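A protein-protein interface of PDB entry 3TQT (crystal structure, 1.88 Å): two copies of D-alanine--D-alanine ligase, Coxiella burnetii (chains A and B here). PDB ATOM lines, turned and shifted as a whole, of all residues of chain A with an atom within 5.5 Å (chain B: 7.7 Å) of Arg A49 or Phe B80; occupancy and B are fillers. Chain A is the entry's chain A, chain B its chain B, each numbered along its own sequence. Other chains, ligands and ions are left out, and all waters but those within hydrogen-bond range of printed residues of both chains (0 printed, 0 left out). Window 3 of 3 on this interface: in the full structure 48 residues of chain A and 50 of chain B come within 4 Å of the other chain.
The side-chain carboxylate of Asp A45 lies within hydrogen-bond range of the backbone NH of Gly A48 (2.9 Å). The guanidinium group (NE) of Arg A49 is in salt-bridge range of the side-chain carboxylate (OD2) of Asp A45, at 2.9 Å. The backbone carbonyl oxygen (O) of Trp A50 is in hydrogen-bond range of the backbone NH (N) of Ile A76, at 3.0 Å. The backbone NH (N) of Thr B77 is in hydrogen-bond range of the backbone carbonyl oxygen (O) of Gln B88 (2.8 Å).
Of chain B, only Phe B80 comes within 4 Å of Arg A49. Of chain A, only Gly A48, Arg A49, Trp A50, Ile A78 and Leu A119 come within 4 Å of Phe B80. Gly A48 touches one residue of chain B. Of the printed residues of chain A, Leu B122 touches Leu A119 (3.7 Å). Of the printed residues of chain B, Ile A78 touches Thr B77, Ile B78 and Phe B80. The nearest residue of chain B that does not touch Arg A49 is Ala B79 (7.2 Å). The nearest printed residue of chain A that does not touch Ile B78 is Leu A119 (4.8 Å).
OG1 of Thr A77 is in hydrogen-bond range of OG1 of Thr B77, 3.3 Å away. O of Ile B78 lies within hydrogen-bond range of OG1 of Thr A77 (2.4 Å). O of Ile A78 sits close to OG1 of Thr B77 (2.3 Å).
Thr A77 touches its own counterpart, Thr B77. Thr A77 touches Ile B78, and with the chains exchanged Ile A78 touches Thr B77. Ile A78 touches its own counterpart, Ile B78. Leu A119 touches its own counterpart, Leu B119. Of the 11 pairs that touch across the chains among the printed residues, 5 have their exchanged pair printed and touching as well.
Printed residues of chain A that touch a printed residue of chain B: Gly A48, Arg A49, Trp A50, Thr A77, Ile A78 and Leu A119. Hydrophobic or aromatic side chains of chain A within 4 Å of the printed part of chain B: Trp A50, Ile A78 and Leu A119. Among the printed residues, no Asp or Glu carboxylate lies within 4 Å of a Lys or Arg side-chain nitrogen of the other chain.
Phe B80 touches Gly A48 (CB to O, 3.2 Å). Phe B80 touches Arg A49 (O to CG, 3.9 Å). CD1 of Trp A50 touches CG of Phe B80, 3.5 Å away. CD1 of Ile B78 touches CD1 of Ile A78, at 3.3 Å. CE2 of Phe B80 touches CG2 of Ile A78 (3.9 Å). Phe B80 touches Leu A119. Leu B119 touches Leu A119. Leu A119 touches Leu B122.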
ATOM      1  N   PHE A  43       0.148 -35.134  14.800  1.00  0.00           N
ATOM      2  CA  PHE A  43      -0.809 -35.735  15.712  1.00  0.00           C
ATOM      3  C   PHE A  43      -1.082 -34.802  16.879  1.00  0.00           C
ATOM      4  O   PHE A  43      -0.157 -34.348  17.539  1.00  0.00           O
ATOM      5  CB  PHE A  43      -0.268 -37.072  16.234  1.00  0.00           C
ATOM      6  CG  PHE A  43      -1.177 -37.753  17.217  1.00  0.00           C
ATOM      7  CD1 PHE A  43      -2.471 -38.093  16.859  1.00  0.00           C
ATOM      8  CD2 PHE A  43      -0.733 -38.060  18.498  1.00  0.00           C
ATOM      9  CE1 PHE A  43      -3.306 -38.733  17.752  1.00  0.00           C
ATOM     10  CE2 PHE A  43      -1.565 -38.696  19.400  1.00  0.00           C
ATOM     11  CZ  PHE A  43      -2.855 -39.036  19.027  1.00  0.00           C
ATOM     12  N   ILE A  44      -2.358 -34.519  17.122  1.00  0.00           N
ATOM     13  CA  ILE A  44      -2.762 -33.738  18.275  1.00  0.00           C
ATOM     14  C   ILE A  44      -3.399 -34.708  19.239  1.00  0.00           C
ATOM     15  O   ILE A  44      -4.404 -35.331  18.908  1.00  0.00           O
ATOM     16  CB  ILE A  44      -3.801 -32.675  17.888  1.00  0.00           C
ATOM     17  CG1 ILE A  44      -3.248 -31.792  16.758  1.00  0.00           C
ATOM     18  CG2 ILE A  44      -4.223 -31.862  19.113  1.00  0.00           C
ATOM     19  CD1 ILE A  44      -4.205 -30.717  16.289  1.00  0.00           C
ATOM     20  N   ASP A  45      -2.821 -34.858  20.424  1.00  0.00           N
ATOM     21  CA  ASP A  45      -3.364 -35.831  21.361  1.00  0.00           C
ATOM     22  C   ASP A  45      -4.575 -35.283  22.107  1.00  0.00           C
ATOM     23  O   ASP A  45      -5.077 -34.195  21.805  1.00  0.00           O
ATOM     24  CB  ASP A  45      -2.290 -36.340  22.333  1.00  0.00           C
ATOM     25  CG  ASP A  45      -1.831 -35.282  23.322  1.00  0.00           C
ATOM     26  OD1 ASP A  45      -2.503 -34.235  23.456  1.00  0.00           O
ATOM     27  OD2 ASP A  45      -0.794 -35.516  23.982  1.00  0.00           O
ATOM     28  N   VAL A  47      -5.023 -34.099  25.062  1.00  0.00           N
ATOM     29  CA  VAL A  47      -4.867 -32.874  25.840  1.00  0.00           C
ATOM     30  C   VAL A  47      -4.371 -31.716  24.982  1.00  0.00           C
ATOM     31  O   VAL A  47      -4.051 -30.647  25.496  1.00  0.00           O
ATOM     32  CB  VAL A  47      -3.935 -33.061  27.056  1.00  0.00           C
ATOM     33  CG1 VAL A  47      -4.476 -34.149  27.975  1.00  0.00           C
ATOM     34  CG2 VAL A  47      -2.525 -33.388  26.605  1.00  0.00           C
ATOM     35  N   GLY A  48      -4.300 -31.932  23.673  1.00  0.00           N
ATOM     36  CA  GLY A  48      -3.976 -30.856  22.756  1.00  0.00           C
ATOM     37  C   GLY A  48      -2.498 -30.648  22.500  1.00  0.00           C
ATOM     38  O   GLY A  48      -2.096 -29.600  22.003  1.00  0.00           O
ATOM     39  N   ARG A  49      -1.683 -31.636  22.843  1.00  0.00           N
ATOM     40  CA  ARG A  49      -0.260 -31.582  22.517  1.00  0.00           C
ATOM     41  C   ARG A  49      -0.022 -32.024  21.078  1.00  0.00           C
ATOM     42  O   ARG A  49      -0.658 -32.963  20.600  1.00  0.00           O
ATOM     43  CB  ARG A  49       0.543 -32.467  23.468  1.00  0.00           C
ATOM     44  CG  ARG A  49       0.674 -31.887  24.862  1.00  0.00           C
ATOM     45  CD  ARG A  49       1.374 -32.856  25.809  1.00  0.00           C
ATOM     46  NE  ARG A  49       0.526 -34.004  26.101  1.00  0.00           N
ATOM     47  CZ  ARG A  49       0.747 -34.867  27.084  1.00  0.00           C
ATOM     48  NH1 ARG A  49       1.798 -34.715  27.881  1.00  0.00           N
ATOM     49  NH2 ARG A  49      -0.088 -35.879  27.270  1.00  0.00           N
ATOM     50  N   TRP A  50       0.897 -31.348  20.395  1.00  0.00           N
ATOM     51  CA  TRP A  50       1.182 -31.652  18.998  1.00  0.00           C
ATOM     52  C   TRP A  50       2.466 -32.439  18.828  1.00  0.00           C
ATOM     53  O   TRP A  50       3.481 -32.153  19.464  1.00  0.00           O
ATOM     54  CB  TRP A  50       1.316 -30.368  18.178  1.00  0.00           C
ATOM     55  CG  TRP A  50       0.053 -29.620  17.969  1.00  0.00           C
ATOM     56  CD1 TRP A  50      -0.963 -29.454  18.854  1.00  0.00           C
ATOM     57  CD2 TRP A  50      -0.332 -28.923  16.773  1.00  0.00           C
ATOM     58  NE1 TRP A  50      -1.957 -28.687  18.292  1.00  0.00           N
ATOM     59  CE2 TRP A  50      -1.595 -28.354  17.016  1.00  0.00           C
ATOM     60  CE3 TRP A  50       0.273 -28.729  15.528  1.00  0.00           C
ATOM     61  CZ2 TRP A  50      -2.277 -27.603  16.048  1.00  0.00           C
ATOM     62  CZ3 TRP A  50      -0.397 -27.981  14.572  1.00  0.00           C
ATOM     63  CH2 TRP A  50      -1.661 -27.429  14.837  1.00  0.00           C
ATOM     64  N   TYR A  51       2.419 -33.413  17.929  1.00  0.00           N
ATOM     65  CA  TYR A  51       3.573 -34.230  17.628  1.00  0.00           C
ATOM     66  C   TYR A  51       3.700 -34.334  16.122  1.00  0.00           C
ATOM     67  O   TYR A  51       2.707 -34.357  15.408  1.00  0.00           O
ATOM     68  CB  TYR A  51       3.429 -35.620  18.228  1.00  0.00           C
ATOM     69  CG  TYR A  51       3.197 -35.647  19.728  1.00  0.00           C
ATOM     70  CD1 TYR A  51       4.263 -35.733  20.613  1.00  0.00           C
ATOM     71  CD2 TYR A  51       1.912 -35.596  20.254  1.00  0.00           C
ATOM     72  CE1 TYR A  51       4.063 -35.767  21.976  1.00  0.00           C
ATOM     73  CE2 TYR A  51       1.702 -35.638  21.627  1.00  0.00           C
ATOM     74  CZ  TYR A  51       2.782 -35.723  22.478  1.00  0.00           C
ATOM     75  OH  TYR A  51       2.589 -35.750  23.837  1.00  0.00           O
ATOM     76  N   ILE A  76       6.176 -31.034  18.930  1.00  0.00           N
ATOM     77  CA  ILE A  76       6.455 -29.830  18.174  1.00  0.00           C
ATOM     78  C   ILE A  76       5.622 -28.674  18.668  1.00  0.00           C
ATOM     79  O   ILE A  76       4.592 -28.847  19.329  1.00  0.00           O
ATOM     80  CB  ILE A  76       6.172 -30.001  16.677  1.00  0.00           C
ATOM     81  CG1 ILE A  76       4.748 -30.539  16.459  1.00  0.00           C
ATOM     82  CG2 ILE A  76       7.240 -30.881  16.017  1.00  0.00           C
ATOM     83  CD1 ILE A  76       4.173 -30.181  15.082  1.00  0.00           C
ATOM     84  N   THR A  77       6.090 -27.479  18.354  1.00  0.00           N
ATOM     85  CA  THR A  77       5.225 -26.330  18.419  1.00  0.00           C
ATOM     86  C   THR A  77       5.289 -25.654  17.060  1.00  0.00           C
ATOM     87  O   THR A  77       5.716 -26.265  16.089  1.00  0.00           O
ATOM     88  CB  THR A  77       5.587 -25.387  19.559  1.00  0.00           C
ATOM     89  OG1 THR A  77       4.621 -24.331  19.602  1.00  0.00           O
ATOM     90  CG2 THR A  77       6.991 -24.816  19.375  1.00  0.00           C
ATOM     91  N   ILE A  78       4.842 -24.415  16.972  1.00  0.00           N
ATOM     92  CA  ILE A  78       4.788 -23.765  15.681  1.00  0.00           C
ATOM     93  C   ILE A  78       5.750 -22.590  15.647  1.00  0.00           C
ATOM     94  O   ILE A  78       6.145 -22.065  16.678  1.00  0.00           O
ATOM     95  CB  ILE A  78       3.350 -23.322  15.307  1.00  0.00           C
ATOM     96  CG1 ILE A  78       2.814 -22.329  16.325  1.00  0.00           C
ATOM     97  CG2 ILE A  78       2.428 -24.528  15.199  1.00  0.00           C
ATOM     98  CD1 ILE A  78       1.389 -21.927  16.069  1.00  0.00           C
ATOM     99  N   LEU A 119      -5.598 -21.076  13.088  1.00  0.00           N
ATOM    100  CA  LEU A 119      -4.170 -21.199  13.354  1.00  0.00           C
ATOM    101  C   LEU A 119      -3.415 -21.241  12.037  1.00  0.00           C
ATOM    102  O   LEU A 119      -2.375 -20.592  11.872  1.00  0.00           O
ATOM    103  CB  LEU A 119      -3.872 -22.457  14.172  1.00  0.00           C
ATOM    104  CG  LEU A 119      -2.382 -22.750  14.348  1.00  0.00           C
ATOM    105  CD1 LEU A 119      -1.651 -21.484  14.780  1.00  0.00           C
ATOM    106  CD2 LEU A 119      -2.181 -23.889  15.356  1.00  0.00           C
ATOM    107  N   THR B  77       6.708 -18.444  20.740  1.00  0.00           N
ATOM    108  CA  THR B  77       5.764 -19.306  20.070  1.00  0.00           C
ATOM    109  C   THR B  77       4.762 -19.753  21.116  1.00  0.00           C
ATOM    110  O   THR B  77       4.714 -19.208  22.215  1.00  0.00           O
ATOM    111  CB  THR B  77       6.427 -20.525  19.433  1.00  0.00           C
ATOM    112  OG1 THR B  77       5.430 -21.267  18.726  1.00  0.00           O
ATOM    113  CG2 THR B  77       7.050 -21.423  20.499  1.00  0.00           C
ATOM    114  N   ILE B  78       3.960 -20.747  20.788  1.00  0.00           N
ATOM    115  CA  ILE B  78       2.972 -21.188  21.743  1.00  0.00           C
ATOM    116  C   ILE B  78       3.371 -22.527  22.316  1.00  0.00           C
ATOM    117  O   ILE B  78       4.144 -23.271  21.722  1.00  0.00           O
ATOM    118  CB  ILE B  78       1.568 -21.234  21.119  1.00  0.00           C
ATOM    119  CG1 ILE B  78       1.563 -22.113  19.881  1.00  0.00           C
ATOM    120  CG2 ILE B  78       1.120 -19.824  20.732  1.00  0.00           C
ATOM    121  CD1 ILE B  78       0.258 -22.048  19.137  1.00  0.00           C
ATOM    122  N   ALA B  79       2.876 -22.825  23.498  1.00  0.00           N
ATOM    123  CA  ALA B  79       3.078 -24.153  24.038  1.00  0.00           C
ATOM    124  C   ALA B  79       1.704 -24.793  24.038  1.00  0.00           C
ATOM    125  O   ALA B  79       0.792 -24.299  24.690  1.00  0.00           O
ATOM    126  CB  ALA B  79       3.649 -24.081  25.438  1.00  0.00           C
ATOM    127  N   PHE B  80       1.536 -25.862  23.271  1.00  0.00           N
ATOM    128  CA  PHE B  80       0.242 -26.525  23.188  1.00  0.00           C
ATOM    129  C   PHE B  80      -0.046 -27.377  24.424  1.00  0.00           C
ATOM    130  O   PHE B  80       0.861 -28.006  24.971  1.00  0.00           O
ATOM    131  CB  PHE B  80       0.177 -27.393  21.944  1.00  0.00           C
ATOM    132  CG  PHE B  80       0.022 -26.623  20.679  1.00  0.00           C
ATOM    133  CD1 PHE B  80      -1.135 -25.909  20.424  1.00  0.00           C
ATOM    134  CD2 PHE B  80       1.023 -26.629  19.726  1.00  0.00           C
ATOM    135  CE1 PHE B  80      -1.286 -25.206  19.244  1.00  0.00           C
ATOM    136  CE2 PHE B  80       0.874 -25.928  18.547  1.00  0.00           C
ATOM    137  CZ  PHE B  80      -0.282 -25.222  18.306  1.00  0.00           C
ATOM    138  N   LYS B  85       0.075 -21.695  30.811  1.00  0.00           N
ATOM    139  CA  LYS B  85       1.303 -21.110  30.292  1.00  0.00           C
ATOM    140  C   LYS B  85       1.416 -21.384  28.806  1.00  0.00           C
ATOM    141  O   LYS B  85       2.164 -22.272  28.384  1.00  0.00           O
ATOM    142  CB  LYS B  85       2.523 -21.650  31.037  1.00  0.00           C
ATOM    143  CG  LYS B  85       2.535 -21.301  32.517  1.00  0.00           C
ATOM    144  CD  LYS B  85       3.956 -21.130  33.034  1.00  0.00           C
ATOM    145  CE  LYS B  85       3.965 -20.512  34.424  1.00  0.00           C
ATOM    146  NZ  LYS B  85       5.324 -20.079  34.851  1.00  0.00           N
ATOM    147  N   PRO B  86       0.653 -20.618  28.010  1.00  0.00           N
ATOM    148  CA  PRO B  86       0.519 -20.785  26.559  1.00  0.00           C
ATOM    149  C   PRO B  86       1.676 -20.212  25.759  1.00  0.00           C
ATOM    150  O   PRO B  86       1.875 -20.656  24.634  1.00  0.00           O
ATOM    151  CB  PRO B  86      -0.770 -20.014  26.237  1.00  0.00           C
ATOM    152  CG  PRO B  86      -0.814 -18.935  27.274  1.00  0.00           C
ATOM    153  CD  PRO B  86      -0.232 -19.553  28.526  1.00  0.00           C
ATOM    154  N   TRP B  87       2.424 -19.252  26.302  1.00  0.00           N
ATOM    155  CA  TRP B  87       3.492 -18.648  25.520  1.00  0.00           C
ATOM    156  C   TRP B  87       4.850 -19.227  25.920  1.00  0.00           C
ATOM    157  O   TRP B  87       5.115 -19.494  27.091  1.00  0.00           O
ATOM    158  CB  TRP B  87       3.520 -17.120  25.667  1.00  0.00           C
ATOM    159  CG  TRP B  87       2.168 -16.464  25.773  1.00  0.00           C
ATOM    160  CD1 TRP B  87       1.746 -15.619  26.757  1.00  0.00           C
ATOM    161  CD2 TRP B  87       1.076 -16.593  24.857  1.00  0.00           C
ATOM    162  NE1 TRP B  87       0.461 -15.214  26.513  1.00  0.00           N
ATOM    163  CE2 TRP B  87       0.021 -15.795  25.355  1.00  0.00           C
ATOM    164  CE3 TRP B  87       0.882 -17.303  23.671  1.00  0.00           C
ATOM    165  CZ2 TRP B  87      -1.210 -15.700  24.714  1.00  0.00           C
ATOM    166  CZ3 TRP B  87      -0.347 -17.199  23.022  1.00  0.00           C
ATOM    167  CH2 TRP B  87      -1.376 -16.404  23.548  1.00  0.00           C
ATOM    168  N   GLN B  88       5.703 -19.427  24.931  1.00  0.00           N
ATOM    169  CA  GLN B  88       7.033 -19.976  25.169  1.00  0.00           C
ATOM    170  C   GLN B  88       8.065 -19.191  24.381  1.00  0.00           C
ATOM    171  O   GLN B  88       7.866 -18.898  23.202  1.00  0.00           O
ATOM    172  CB  GLN B  88       7.078 -21.448  24.770  1.00  0.00           C
ATOM    173  CG  GLN B  88       8.472 -22.017  24.723  1.00  0.00           C
ATOM    174  CD  GLN B  88       8.484 -23.502  24.991  1.00  0.00           C
ATOM    175  OE1 GLN B  88       7.611 -24.227  24.524  1.00  0.00           O
ATOM    176  NE2 GLN B  88       9.463 -23.964  25.770  1.00  0.00           N
ATOM    177  N   ARG B  96       8.516 -20.326  29.746  1.00  0.00           N
ATOM    178  CA  ARG B  96       7.088 -20.270  29.443  1.00  0.00           C
ATOM    179  C   ARG B  96       6.427 -19.155  30.245  1.00  0.00           C
ATOM    180  O   ARG B  96       6.842 -18.861  31.367  1.00  0.00           O
ATOM    181  CB  ARG B  96       6.432 -21.622  29.725  1.00  0.00           C
ATOM    182  CG  ARG B  96       7.091 -22.773  28.970  1.00  0.00           C
ATOM    183  CD  ARG B  96       6.146 -23.953  28.769  1.00  0.00           C
ATOM    184  NE  ARG B  96       6.490 -24.709  27.566  1.00  0.00           N
ATOM    185  CZ  ARG B  96       5.916 -25.852  27.203  1.00  0.00           C
ATOM    186  NH1 ARG B  96       4.962 -26.385  27.956  1.00  0.00           N
ATOM    187  NH2 ARG B  96       6.295 -26.466  26.088  1.00  0.00           N
ATOM    188  N   LEU B 119      -7.113 -19.846  17.322  1.00  0.00           N
ATOM    189  CA  LEU B 119      -5.894 -20.236  18.024  1.00  0.00           C
ATOM    190  C   LEU B 119      -6.132 -20.242  19.527  1.00  0.00           C
ATOM    191  O   LEU B 119      -5.695 -21.155  20.245  1.00  0.00           O
ATOM    192  CB  LEU B 119      -4.718 -19.313  17.679  1.00  0.00           C
ATOM    193  CG  LEU B 119      -3.474 -19.578  18.540  1.00  0.00           C
ATOM    194  CD1 LEU B 119      -2.944 -20.995  18.307  1.00  0.00           C
ATOM    195  CD2 LEU B 119      -2.388 -18.556  18.302  1.00  0.00           C
ATOM    196  N   LEU B 122      -7.994 -23.285  20.424  1.00  0.00           N
ATOM    197  CA  LEU B 122      -7.082 -24.432  20.427  1.00  0.00           C
ATOM    198  C   LEU B 122      -6.237 -24.492  21.692  1.00  0.00           C
ATOM    199  O   LEU B 122      -5.848 -25.566  22.132  1.00  0.00           O
ATOM    200  CB  LEU B 122      -6.135 -24.390  19.228  1.00  0.00           C
ATOM    201  CG  LEU B 122      -6.631 -24.837  17.861  1.00  0.00           C
ATOM    202  CD1 LEU B 122      -5.561 -24.532  16.813  1.00  0.00           C
ATOM    203  CD2 LEU B 122      -6.960 -26.327  17.898  1.00  0.00           C
ATOM    204  N   LEU B 123      -5.923 -23.329  22.251  1.00  0.00           N
ATOM    205  CA  LEU B 123      -5.075 -23.259  23.433  1.00  0.00           C
ATOM    206  C   LEU B 123      -5.881 -23.322  24.726  1.00  0.00           C
ATOM    207  O   LEU B 123      -5.311 -23.239  25.813  1.00  0.00           O
ATOM    208  CB  LEU B 123      -4.226 -21.985  23.399  1.00  0.00           C
ATOM    209  CG  LEU B 123      -3.130 -21.965  22.329  1.00  0.00           C
ATOM    210  CD1 LEU B 123      -2.440 -20.612  22.271  1.00  0.00           C
ATOM    211  CD2 LEU B 123      -2.125 -23.076  22.590  1.00  0.00           C
